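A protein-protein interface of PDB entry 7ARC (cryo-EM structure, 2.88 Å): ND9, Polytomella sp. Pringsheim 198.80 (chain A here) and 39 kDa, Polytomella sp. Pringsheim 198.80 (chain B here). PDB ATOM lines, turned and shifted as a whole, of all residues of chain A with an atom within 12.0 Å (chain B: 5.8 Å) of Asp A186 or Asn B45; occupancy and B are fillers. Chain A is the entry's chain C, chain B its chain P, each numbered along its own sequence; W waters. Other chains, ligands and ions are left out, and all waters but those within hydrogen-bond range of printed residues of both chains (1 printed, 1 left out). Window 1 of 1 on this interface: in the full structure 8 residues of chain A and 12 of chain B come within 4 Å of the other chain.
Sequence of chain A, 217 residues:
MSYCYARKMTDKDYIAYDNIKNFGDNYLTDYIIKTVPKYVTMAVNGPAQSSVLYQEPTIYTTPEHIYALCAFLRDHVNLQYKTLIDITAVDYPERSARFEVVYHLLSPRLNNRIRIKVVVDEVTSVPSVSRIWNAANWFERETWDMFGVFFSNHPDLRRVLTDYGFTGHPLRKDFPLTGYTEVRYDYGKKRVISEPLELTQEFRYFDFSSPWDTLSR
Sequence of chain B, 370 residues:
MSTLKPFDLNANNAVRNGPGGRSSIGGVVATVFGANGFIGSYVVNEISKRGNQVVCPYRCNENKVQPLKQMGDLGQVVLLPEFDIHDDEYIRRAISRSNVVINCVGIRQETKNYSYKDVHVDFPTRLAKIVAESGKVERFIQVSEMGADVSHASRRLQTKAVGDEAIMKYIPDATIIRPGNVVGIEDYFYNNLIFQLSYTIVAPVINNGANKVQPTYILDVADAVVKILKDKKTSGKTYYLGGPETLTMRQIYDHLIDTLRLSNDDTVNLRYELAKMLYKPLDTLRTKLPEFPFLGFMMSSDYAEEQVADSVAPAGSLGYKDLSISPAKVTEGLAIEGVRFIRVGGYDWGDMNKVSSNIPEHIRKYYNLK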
ATOM      1  N   GLU A 182     -20.326 -38.706  15.722  1.00  0.00           N
ATOM      2  CA  GLU A 182     -18.893 -38.941  15.721  1.00  0.00           C
ATOM      3  C   GLU A 182     -18.246 -38.001  16.723  1.00  0.00           C
ATOM      4  O   GLU A 182     -18.782 -36.940  17.042  1.00  0.00           O
ATOM      5  CB  GLU A 182     -18.299 -38.723  14.327  1.00  0.00           C
ATOM      6  CG  GLU A 182     -17.158 -39.647  13.979  1.00  0.00           C
ATOM      7  CD  GLU A 182     -16.642 -39.419  12.573  1.00  0.00           C
ATOM      8  OE1 GLU A 182     -17.166 -38.518  11.887  1.00  0.00           O
ATOM      9  OE2 GLU A 182     -15.716 -40.143  12.153  1.00  0.00           O
ATOM     10  N   VAL A 183     -17.078 -38.401  17.213  1.00  0.00           N
ATOM     11  CA  VAL A 183     -16.412 -37.740  18.328  1.00  0.00           C
ATOM     12  C   VAL A 183     -15.099 -37.159  17.828  1.00  0.00           C
ATOM     13  O   VAL A 183     -14.328 -37.847  17.151  1.00  0.00           O
ATOM     14  CB  VAL A 183     -16.189 -38.703  19.505  1.00  0.00           C
ATOM     15  CG1 VAL A 183     -15.406 -38.032  20.588  1.00  0.00           C
ATOM     16  CG2 VAL A 183     -17.526 -39.135  20.062  1.00  0.00           C
ATOM     17  N   ARG A 184     -14.849 -35.898  18.166  1.00  0.00           N
ATOM     18  CA  ARG A 184     -13.657 -35.192  17.728  1.00  0.00           C
ATOM     19  C   ARG A 184     -13.267 -34.173  18.784  1.00  0.00           C
ATOM     20  O   ARG A 184     -14.119 -33.662  19.513  1.00  0.00           O
ATOM     21  CB  ARG A 184     -13.919 -34.489  16.394  1.00  0.00           C
ATOM     22  CG  ARG A 184     -12.742 -33.769  15.796  1.00  0.00           C
ATOM     23  CD  ARG A 184     -13.148 -33.127  14.493  1.00  0.00           C
ATOM     24  NE  ARG A 184     -14.177 -32.116  14.705  1.00  0.00           N
ATOM     25  CZ  ARG A 184     -13.932 -30.868  15.080  1.00  0.00           C
ATOM     26  NH1 ARG A 184     -12.698 -30.437  15.282  1.00  0.00           N
ATOM     27  NH2 ARG A 184     -14.949 -30.030  15.253  1.00  0.00           N
ATOM     28  N   TYR A 185     -11.974 -33.881  18.866  1.00  0.00           N
ATOM     29  CA  TYR A 185     -11.485 -32.805  19.715  1.00  0.00           C
ATOM     30  C   TYR A 185     -11.442 -31.515  18.908  1.00  0.00           C
ATOM     31  O   TYR A 185     -10.966 -31.505  17.769  1.00  0.00           O
ATOM     32  CB  TYR A 185     -10.099 -33.130  20.271  1.00  0.00           C
ATOM     33  CG  TYR A 185      -9.420 -31.960  20.943  1.00  0.00           C
ATOM     34  CD1 TYR A 185      -9.752 -31.597  22.238  1.00  0.00           C
ATOM     35  CD2 TYR A 185      -8.449 -31.223  20.288  1.00  0.00           C
ATOM     36  CE1 TYR A 185      -9.140 -30.535  22.859  1.00  0.00           C
ATOM     37  CE2 TYR A 185      -7.832 -30.156  20.903  1.00  0.00           C
ATOM     38  CZ  TYR A 185      -8.182 -29.816  22.188  1.00  0.00           C
ATOM     39  OH  TYR A 185      -7.569 -28.755  22.807  1.00  0.00           O
ATOM     40  N   ASP A 186     -11.934 -30.432  19.496  1.00  0.00           N
ATOM     41  CA  ASP A 186     -11.905 -29.123  18.863  1.00  0.00           C
ATOM     42  C   ASP A 186     -10.812 -28.273  19.494  1.00  0.00           C
ATOM     43  O   ASP A 186     -10.639 -28.277  20.714  1.00  0.00           O
ATOM     44  CB  ASP A 186     -13.258 -28.427  18.998  1.00  0.00           C
ATOM     45  CG  ASP A 186     -13.461 -27.342  17.965  1.00  0.00           C
ATOM     46  OD1 ASP A 186     -12.585 -27.177  17.091  1.00  0.00           O
ATOM     47  OD2 ASP A 186     -14.498 -26.653  18.026  1.00  0.00           O
ATOM     48  N   TYR A 187     -10.051 -27.567  18.659  1.00  0.00           N
ATOM     49  CA  TYR A 187      -9.030 -26.681  19.205  1.00  0.00           C
ATOM     50  C   TYR A 187      -9.631 -25.404  19.777  1.00  0.00           C
ATOM     51  O   TYR A 187      -9.184 -24.925  20.824  1.00  0.00           O
ATOM     52  CB  TYR A 187      -7.995 -26.341  18.138  1.00  0.00           C
ATOM     53  CG  TYR A 187      -6.849 -25.510  18.663  1.00  0.00           C
ATOM     54  CD1 TYR A 187      -5.881 -26.071  19.483  1.00  0.00           C
ATOM     55  CD2 TYR A 187      -6.742 -24.162  18.352  1.00  0.00           C
ATOM     56  CE1 TYR A 187      -4.835 -25.318  19.969  1.00  0.00           C
ATOM     57  CE2 TYR A 187      -5.698 -23.402  18.833  1.00  0.00           C
ATOM     58  CZ  TYR A 187      -4.748 -23.985  19.641  1.00  0.00           C
ATOM     59  OH  TYR A 187      -3.705 -23.232  20.126  1.00  0.00           O
ATOM     60  N   GLY A 188     -10.624 -24.830  19.101  1.00  0.00           N
ATOM     61  CA  GLY A 188     -11.255 -23.606  19.557  1.00  0.00           C
ATOM     62  C   GLY A 188     -11.843 -23.716  20.946  1.00  0.00           C
ATOM     63  O   GLY A 188     -11.474 -22.971  21.858  1.00  0.00           O
ATOM     64  N   LYS A 189     -12.768 -24.654  21.107  1.00  0.00           N
ATOM     65  CA  LYS A 189     -13.274 -25.061  22.412  1.00  0.00           C
ATOM     66  C   LYS A 189     -12.441 -26.256  22.868  1.00  0.00           C
ATOM     67  O   LYS A 189     -12.500 -27.330  22.267  1.00  0.00           O
ATOM     68  CB  LYS A 189     -14.770 -25.365  22.325  1.00  0.00           C
ATOM     69  CG  LYS A 189     -15.149 -26.555  21.450  1.00  0.00           C
ATOM     70  CD  LYS A 189     -16.640 -26.817  21.434  1.00  0.00           C
ATOM     71  CE  LYS A 189     -17.370 -25.759  20.632  1.00  0.00           C
ATOM     72  NZ  LYS A 189     -17.023 -25.807  19.186  1.00  0.00           N
ATOM     73  N   LYS A 190     -11.649 -26.077  23.924  1.00  0.00           N
ATOM     74  CA  LYS A 190     -10.694 -27.111  24.320  1.00  0.00           C
ATOM     75  C   LYS A 190     -11.414 -28.283  24.992  1.00  0.00           C
ATOM     76  O   LYS A 190     -11.186 -28.628  26.150  1.00  0.00           O
ATOM     77  CB  LYS A 190      -9.637 -26.515  25.239  1.00  0.00           C
ATOM     78  CG  LYS A 190      -9.122 -25.153  24.811  1.00  0.00           C
ATOM     79  CD  LYS A 190      -7.970 -25.280  23.835  1.00  0.00           C
ATOM     80  CE  LYS A 190      -7.408 -23.922  23.471  1.00  0.00           C
ATOM     81  NZ  LYS A 190      -7.835 -23.488  22.117  1.00  0.00           N
ATOM     82  N   ARG A 191     -12.294 -28.905  24.213  1.00  0.00           N
ATOM     83  CA  ARG A 191     -13.132 -30.002  24.663  1.00  0.00           C
ATOM     84  C   ARG A 191     -13.242 -31.044  23.562  1.00  0.00           C
ATOM     85  O   ARG A 191     -13.135 -30.731  22.375  1.00  0.00           O
ATOM     86  CB  ARG A 191     -14.525 -29.510  25.067  1.00  0.00           C
ATOM     87  CG  ARG A 191     -14.542 -28.664  26.321  1.00  0.00           C
ATOM     88  CD  ARG A 191     -15.440 -27.468  26.136  1.00  0.00           C
ATOM     89  NE  ARG A 191     -16.617 -27.805  25.351  1.00  0.00           N
ATOM     90  CZ  ARG A 191     -17.465 -26.912  24.865  1.00  0.00           C
ATOM     91  NH1 ARG A 191     -17.298 -25.617  25.073  1.00  0.00           N
ATOM     92  NH2 ARG A 191     -18.497 -27.326  24.137  1.00  0.00           N
ATOM     93  N   VAL A 192     -13.466 -32.287  23.968  1.00  0.00           N
ATOM     94  CA  VAL A 192     -13.793 -33.363  23.041  1.00  0.00           C
ATOM     95  C   VAL A 192     -15.303 -33.356  22.839  1.00  0.00           C
ATOM     96  O   VAL A 192     -16.066 -33.454  23.807  1.00  0.00           O
ATOM     97  CB  VAL A 192     -13.303 -34.717  23.572  1.00  0.00           C
ATOM     98  CG1 VAL A 192     -13.926 -35.839  22.799  1.00  0.00           C
ATOM     99  CG2 VAL A 192     -11.791 -34.801  23.493  1.00  0.00           C
ATOM    100  N   ILE A 193     -15.740 -33.246  21.584  1.00  0.00           N
ATOM    101  CA  ILE A 193     -17.137 -32.979  21.271  1.00  0.00           C
ATOM    102  C   ILE A 193     -17.667 -34.033  20.310  1.00  0.00           C
ATOM    103  O   ILE A 193     -16.914 -34.704  19.602  1.00  0.00           O
ATOM    104  CB  ILE A 193     -17.334 -31.574  20.667  1.00  0.00           C
ATOM    105  CG1 ILE A 193     -16.569 -31.459  19.350  1.00  0.00           C
ATOM    106  CG2 ILE A 193     -16.883 -30.506  21.640  1.00  0.00           C
ATOM    107  CD1 ILE A 193     -16.881 -30.212  18.571  1.00  0.00           C
ATOM    108  N   SER A 194     -18.990 -34.173  20.301  1.00  0.00           N
ATOM    109  CA  SER A 194     -19.688 -35.091  19.414  1.00  0.00           C
ATOM    110  C   SER A 194     -20.360 -34.316  18.289  1.00  0.00           C
ATOM    111  O   SER A 194     -20.949 -33.257  18.517  1.00  0.00           O
ATOM    112  CB  SER A 194     -20.727 -35.910  20.180  1.00  0.00           C
ATOM    113  OG  SER A 194     -21.427 -36.781  19.311  1.00  0.00           O
ATOM    114  N   GLU A 195     -20.273 -34.849  17.077  1.00  0.00           N
ATOM    115  CA  GLU A 195     -20.771 -34.190  15.882  1.00  0.00           C
ATOM    116  C   GLU A 195     -21.503 -35.202  15.017  1.00  0.00           C
ATOM    117  O   GLU A 195     -21.311 -36.412  15.176  1.00  0.00           O
ATOM    118  CB  GLU A 195     -19.624 -33.564  15.076  1.00  0.00           C
ATOM    119  CG  GLU A 195     -18.935 -32.405  15.756  1.00  0.00           C
ATOM    120  CD  GLU A 195     -17.832 -31.819  14.903  1.00  0.00           C
ATOM    121  OE1 GLU A 195     -17.578 -32.362  13.810  1.00  0.00           O
ATOM    122  OE2 GLU A 195     -17.224 -30.811  15.321  1.00  0.00           O
ATOM    123  N   PRO A 196     -22.358 -34.741  14.102  1.00  0.00           N
ATOM    124  CA  PRO A 196     -22.991 -35.668  13.157  1.00  0.00           C
ATOM    125  C   PRO A 196     -21.958 -36.382  12.299  1.00  0.00           C
ATOM    126  O   PRO A 196     -20.861 -35.877  12.053  1.00  0.00           O
ATOM    127  CB  PRO A 196     -23.898 -34.760  12.319  1.00  0.00           C
ATOM    128  CG  PRO A 196     -24.106 -33.556  13.162  1.00  0.00           C
ATOM    129  CD  PRO A 196     -22.828 -33.361  13.902  1.00  0.00           C
ATOM    130  N   GLY B  40      -2.832 -17.174  14.713  1.00  0.00           N
ATOM    131  CA  GLY B  40      -2.811 -18.002  13.520  1.00  0.00           C
ATOM    132  C   GLY B  40      -3.416 -19.375  13.736  1.00  0.00           C
ATOM    133  O   GLY B  40      -4.054 -19.926  12.836  1.00  0.00           O
ATOM    134  N   SER B  41      -3.210 -19.955  14.920  1.00  0.00           N
ATOM    135  CA  SER B  41      -3.700 -21.305  15.174  1.00  0.00           C
ATOM    136  C   SER B  41      -5.219 -21.367  15.098  1.00  0.00           C
ATOM    137  O   SER B  41      -5.781 -22.313  14.540  1.00  0.00           O
ATOM    138  CB  SER B  41      -3.219 -21.790  16.540  1.00  0.00           C
ATOM    139  OG  SER B  41      -1.853 -22.149  16.504  1.00  0.00           O
ATOM    140  N   TYR B  42      -5.903 -20.367  15.652  1.00  0.00           N
ATOM    141  CA  TYR B  42      -7.361 -20.365  15.618  1.00  0.00           C
ATOM    142  C   TYR B  42      -7.890 -20.135  14.208  1.00  0.00           C
ATOM    143  O   TYR B  42      -8.904 -20.721  13.818  1.00  0.00           O
ATOM    144  CB  TYR B  42      -7.893 -19.320  16.593  1.00  0.00           C
ATOM    145  CG  TYR B  42      -7.764 -19.766  18.029  1.00  0.00           C
ATOM    146  CD1 TYR B  42      -6.589 -19.559  18.732  1.00  0.00           C
ATOM    147  CD2 TYR B  42      -8.807 -20.409  18.674  1.00  0.00           C
ATOM    148  CE1 TYR B  42      -6.458 -19.969  20.037  1.00  0.00           C
ATOM    149  CE2 TYR B  42      -8.684 -20.823  19.981  1.00  0.00           C
ATOM    150  CZ  TYR B  42      -7.507 -20.600  20.658  1.00  0.00           C
ATOM    151  OH  TYR B  42      -7.374 -21.010  21.963  1.00  0.00           O
ATOM    152  N   VAL B  43      -7.221 -19.284  13.427  1.00  0.00           N
ATOM    153  CA  VAL B  43      -7.619 -19.081  12.036  1.00  0.00           C
ATOM    154  C   VAL B  43      -7.455 -20.374  11.246  1.00  0.00           C
ATOM    155  O   VAL B  43      -8.322 -20.751  10.445  1.00  0.00           O
ATOM    156  CB  VAL B  43      -6.810 -17.927  11.417  1.00  0.00           C
ATOM    157  CG1 VAL B  43      -6.888 -17.968   9.905  1.00  0.00           C
ATOM    158  CG2 VAL B  43      -7.310 -16.597  11.942  1.00  0.00           C
ATOM    159  N   VAL B  44      -6.339 -21.071  11.465  1.00  0.00           N
ATOM    160  CA  VAL B  44      -6.125 -22.369  10.834  1.00  0.00           C
ATOM    161  C   VAL B  44      -7.215 -23.342  11.248  1.00  0.00           C
ATOM    162  O   VAL B  44      -7.732 -24.104  10.424  1.00  0.00           O
ATOM    163  CB  VAL B  44      -4.724 -22.906  11.181  1.00  0.00           C
ATOM    164  CG1 VAL B  44      -4.620 -24.384  10.855  1.00  0.00           C
ATOM    165  CG2 VAL B  44      -3.658 -22.127  10.439  1.00  0.00           C
ATOM    166  N   ASN B  45      -7.589 -23.329  12.529  1.00  0.00           N
ATOM    167  CA  ASN B  45      -8.640 -24.224  13.000  1.00  0.00           C
ATOM    168  C   ASN B  45      -9.961 -23.943  12.302  1.00  0.00           C
ATOM    169  O   ASN B  45     -10.631 -24.867  11.839  1.00  0.00           O
ATOM    170  CB  ASN B  45      -8.802 -24.089  14.512  1.00  0.00           C
ATOM    171  CG  ASN B  45      -9.830 -25.045  15.070  1.00  0.00           C
ATOM    172  OD1 ASN B  45      -9.713 -26.259  14.916  1.00  0.00           O
ATOM    173  ND2 ASN B  45     -10.848 -24.502  15.721  1.00  0.00           N
ATOM    174  N   GLU B  46     -10.344 -22.670  12.196  1.00  0.00           N
ATOM    175  CA  GLU B  46     -11.601 -22.336  11.531  1.00  0.00           C
ATOM    176  C   GLU B  46     -11.590 -22.747  10.067  1.00  0.00           C
ATOM    177  O   GLU B  46     -12.564 -23.323   9.569  1.00  0.00           O
ATOM    178  CB  GLU B  46     -11.907 -20.848  11.662  1.00  0.00           C
ATOM    179  CG  GLU B  46     -11.823 -20.320  13.064  1.00  0.00           C
ATOM    180  CD  GLU B  46     -12.819 -20.962  14.018  1.00  0.00           C
ATOM    181  OE1 GLU B  46     -13.790 -21.593  13.551  1.00  0.00           O
ATOM    182  OE2 GLU B  46     -12.628 -20.832  15.247  1.00  0.00           O
ATOM    183  N   ILE B  47     -10.509 -22.441   9.348  1.00  0.00           N
ATOM    184  CA  ILE B  47     -10.491 -22.765   7.925  1.00  0.00           C
ATOM    185  C   ILE B  47     -10.477 -24.275   7.710  1.00  0.00           C
ATOM    186  O   ILE B  47     -11.203 -24.798   6.859  1.00  0.00           O
ATOM    187  CB  ILE B  47      -9.300 -22.078   7.233  1.00  0.00           C
ATOM    188  CG1 ILE B  47      -9.393 -20.564   7.404  1.00  0.00           C
ATOM    189  CG2 ILE B  47      -9.255 -22.444   5.764  1.00  0.00           C
ATOM    190  CD1 ILE B  47      -8.171 -19.825   6.934  1.00  0.00           C
ATOM    191  N   SER B  48      -9.673 -25.004   8.486  1.00  0.00           N
ATOM    192  CA  SER B  48      -9.517 -26.435   8.264  1.00  0.00           C
ATOM    193  C   SER B  48     -10.701 -27.236   8.789  1.00  0.00           C
ATOM    194  O   SER B  48     -10.982 -28.325   8.276  1.00  0.00           O
ATOM    195  CB  SER B  48      -8.223 -26.919   8.913  1.00  0.00           C
ATOM    196  OG  SER B  48      -8.059 -28.311   8.737  1.00  0.00           O
ATOM    197  N   LYS B  49     -11.385 -26.726   9.814  1.00  0.00           N
ATOM    198  CA  LYS B  49     -12.543 -27.397  10.389  1.00  0.00           C
ATOM    199  C   LYS B  49     -13.630 -27.643   9.356  1.00  0.00           C
ATOM    200  O   LYS B  49     -14.349 -28.645   9.438  1.00  0.00           O
ATOM    201  CB  LYS B  49     -13.066 -26.548  11.544  1.00  0.00           C
ATOM    202  CG  LYS B  49     -14.241 -27.095  12.295  1.00  0.00           C
ATOM    203  CD  LYS B  49     -14.535 -26.194  13.474  1.00  0.00           C
ATOM    204  CE  LYS B  49     -15.154 -24.893  13.007  1.00  0.00           C
ATOM    205  NZ  LYS B  49     -15.563 -24.031  14.146  1.00  0.00           N
ATOM    206  N   ARG B  50     -13.763 -26.751   8.380  1.00  0.00           N
ATOM    207  CA  ARG B  50     -14.817 -26.817   7.383  1.00  0.00           C
ATOM    208  C   ARG B  50     -14.390 -27.566   6.129  1.00  0.00           C
ATOM    209  O   ARG B  50     -14.989 -27.374   5.066  1.00  0.00           O
ATOM    210  CB  ARG B  50     -15.288 -25.405   7.036  1.00  0.00           C
ATOM    211  CG  ARG B  50     -15.654 -24.600   8.264  1.00  0.00           C
ATOM    212  CD  ARG B  50     -16.003 -23.171   7.933  1.00  0.00           C
ATOM    213  NE  ARG B  50     -16.933 -22.623   8.911  1.00  0.00           N
ATOM    214  CZ  ARG B  50     -16.572 -22.092  10.070  1.00  0.00           C
ATOM    215  NH1 ARG B  50     -15.303 -22.023  10.432  1.00  0.00           N
ATOM    216  NH2 ARG B  50     -17.508 -21.624  10.889  1.00  0.00           N
ATOM    217  N   GLN B  70      -3.552 -32.010  14.337  1.00  0.00           N
ATOM    218  CA  GLN B  70      -4.885 -32.521  14.625  1.00  0.00           C
ATOM    219  C   GLN B  70      -5.991 -31.721  13.942  1.00  0.00           C
ATOM    220  O   GLN B  70      -7.114 -32.221  13.836  1.00  0.00           O
ATOM    221  CB  GLN B  70      -5.084 -32.544  16.148  1.00  0.00           C
ATOM    222  CG  GLN B  70      -6.345 -33.229  16.660  1.00  0.00           C
ATOM    223  CD  GLN B  70      -7.556 -32.320  16.699  1.00  0.00           C
ATOM    224  OE1 GLN B  70      -7.433 -31.110  16.874  1.00  0.00           O
ATOM    225  NE2 GLN B  70      -8.736 -32.902  16.534  1.00  0.00           N
ATOM    226  N   MET B  71      -5.691 -30.519  13.440  1.00  0.00           N
ATOM    227  CA  MET B  71      -6.747 -29.584  13.057  1.00  0.00           C
ATOM    228  C   MET B  71      -7.624 -30.130  11.938  1.00  0.00           C
ATOM    229  O   MET B  71      -8.834 -29.879  11.914  1.00  0.00           O
ATOM    230  CB  MET B  71      -6.139 -28.252  12.627  1.00  0.00           C
ATOM    231  CG  MET B  71      -5.375 -27.533  13.703  1.00  0.00           C
ATOM    232  SD  MET B  71      -6.362 -26.548  14.823  1.00  0.00           S
ATOM    233  CE  MET B  71      -5.066 -25.648  15.661  1.00  0.00           C
HETATM  234  O   HOH W   1     -11.132 -30.767  13.067  1.00  0.00           O
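Of the printed residues of chain A, Asn B45 touches Asp A186, Tyr A187 and Gly A188. Of chain A, only Tyr A187 (3.7 Å) comes within 4 Å of Ser B41. No residue of chain A comes within 4 Å of Val B43. No residue of chain A comes within 4 Å of Ile B47. No residue of chain A comes within 4 Å of Ser B48. Met B71 touches just one residue of chain A: Tyr A187. Printed residues of chain B within 4 Å of Tyr A185: Gln B70. Of the printed residues of chain B, Gly A188 touches Tyr B42 (3.8 Å) and Asn B45 (3.4 Å). Printed residues of chain B within 4 Å of Tyr A187: Ser B41, Tyr B42, Asn B45 and Met B71. Glu A182 touches none of the printed residues of chain B. Arg A184 touches none of the printed residues of chain B. The nearest residue of chain A that does not touch Asn B45 is Arg A184 (5.1 Å). The nearest printed residue of chain B that does not touch Tyr A187 is Gln B70 (4.8 Å).
Among the printed residues, pairs that only touch across the chains: Tyr A187 with Ser B41 (3.7 Å), Tyr A187 with Tyr B42 (3.7 Å), Tyr A187 with Asn B45 (3.7 Å), Tyr A187 with Met B71 (3.5 Å) and Gly A188 with Tyr B42 (3.8 Å).
Hydrophobic or aromatic side chains of chain A that line the printed part of chain B: Tyr A185 and Tyr A187. Among the printed residues, 9 pairs touch across the chains. Among the printed residues, no Asp or Glu carboxylate lies within 4 Å of a Lys or Arg side-chain nitrogen of the other chain.
Water W1 bridges O of Met B71 (2.7 Å) and NH1 of Arg A184 (2.7 Å).
The side-chain amide nitrogen (ND2) of Asn B45 sits close to the backbone NH (N) of Gly A188 (3.4 Å). The side-chain amide nitrogen (ND2) of Asn B45 lies within hydrogen-bond range of the side-chain carboxylate (OD1) of Asp A186, 3.5 Å away. The backbone carbonyl oxygen (O) of Tyr A185 lies within hydrogen-bond range of the side-chain amide nitrogen (NE2) of Gln B70, 2.9 Å away. The side-chain amino group (NZ) of Lys A190 sits at hydrogen-bond distance from the side-chain hydroxyl (OH) of Tyr B42 (2.5 Å).
NH1 of Arg A184 is in salt-bridge range of OD1 of Asp A186, 3.7 Å away. The side-chain carboxylate of Asp A186 lies within salt-bridge range of the side-chain amino group of Lys A189 (2.9 Å). OD1 of Asn B45 lies close to SD of Met B71, at 3.4 Å. The backbone NH (N) of Asp A186 is in hydrogen-bond range of the backbone carbonyl oxygen (O) of Arg A191 (3.1 Å).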
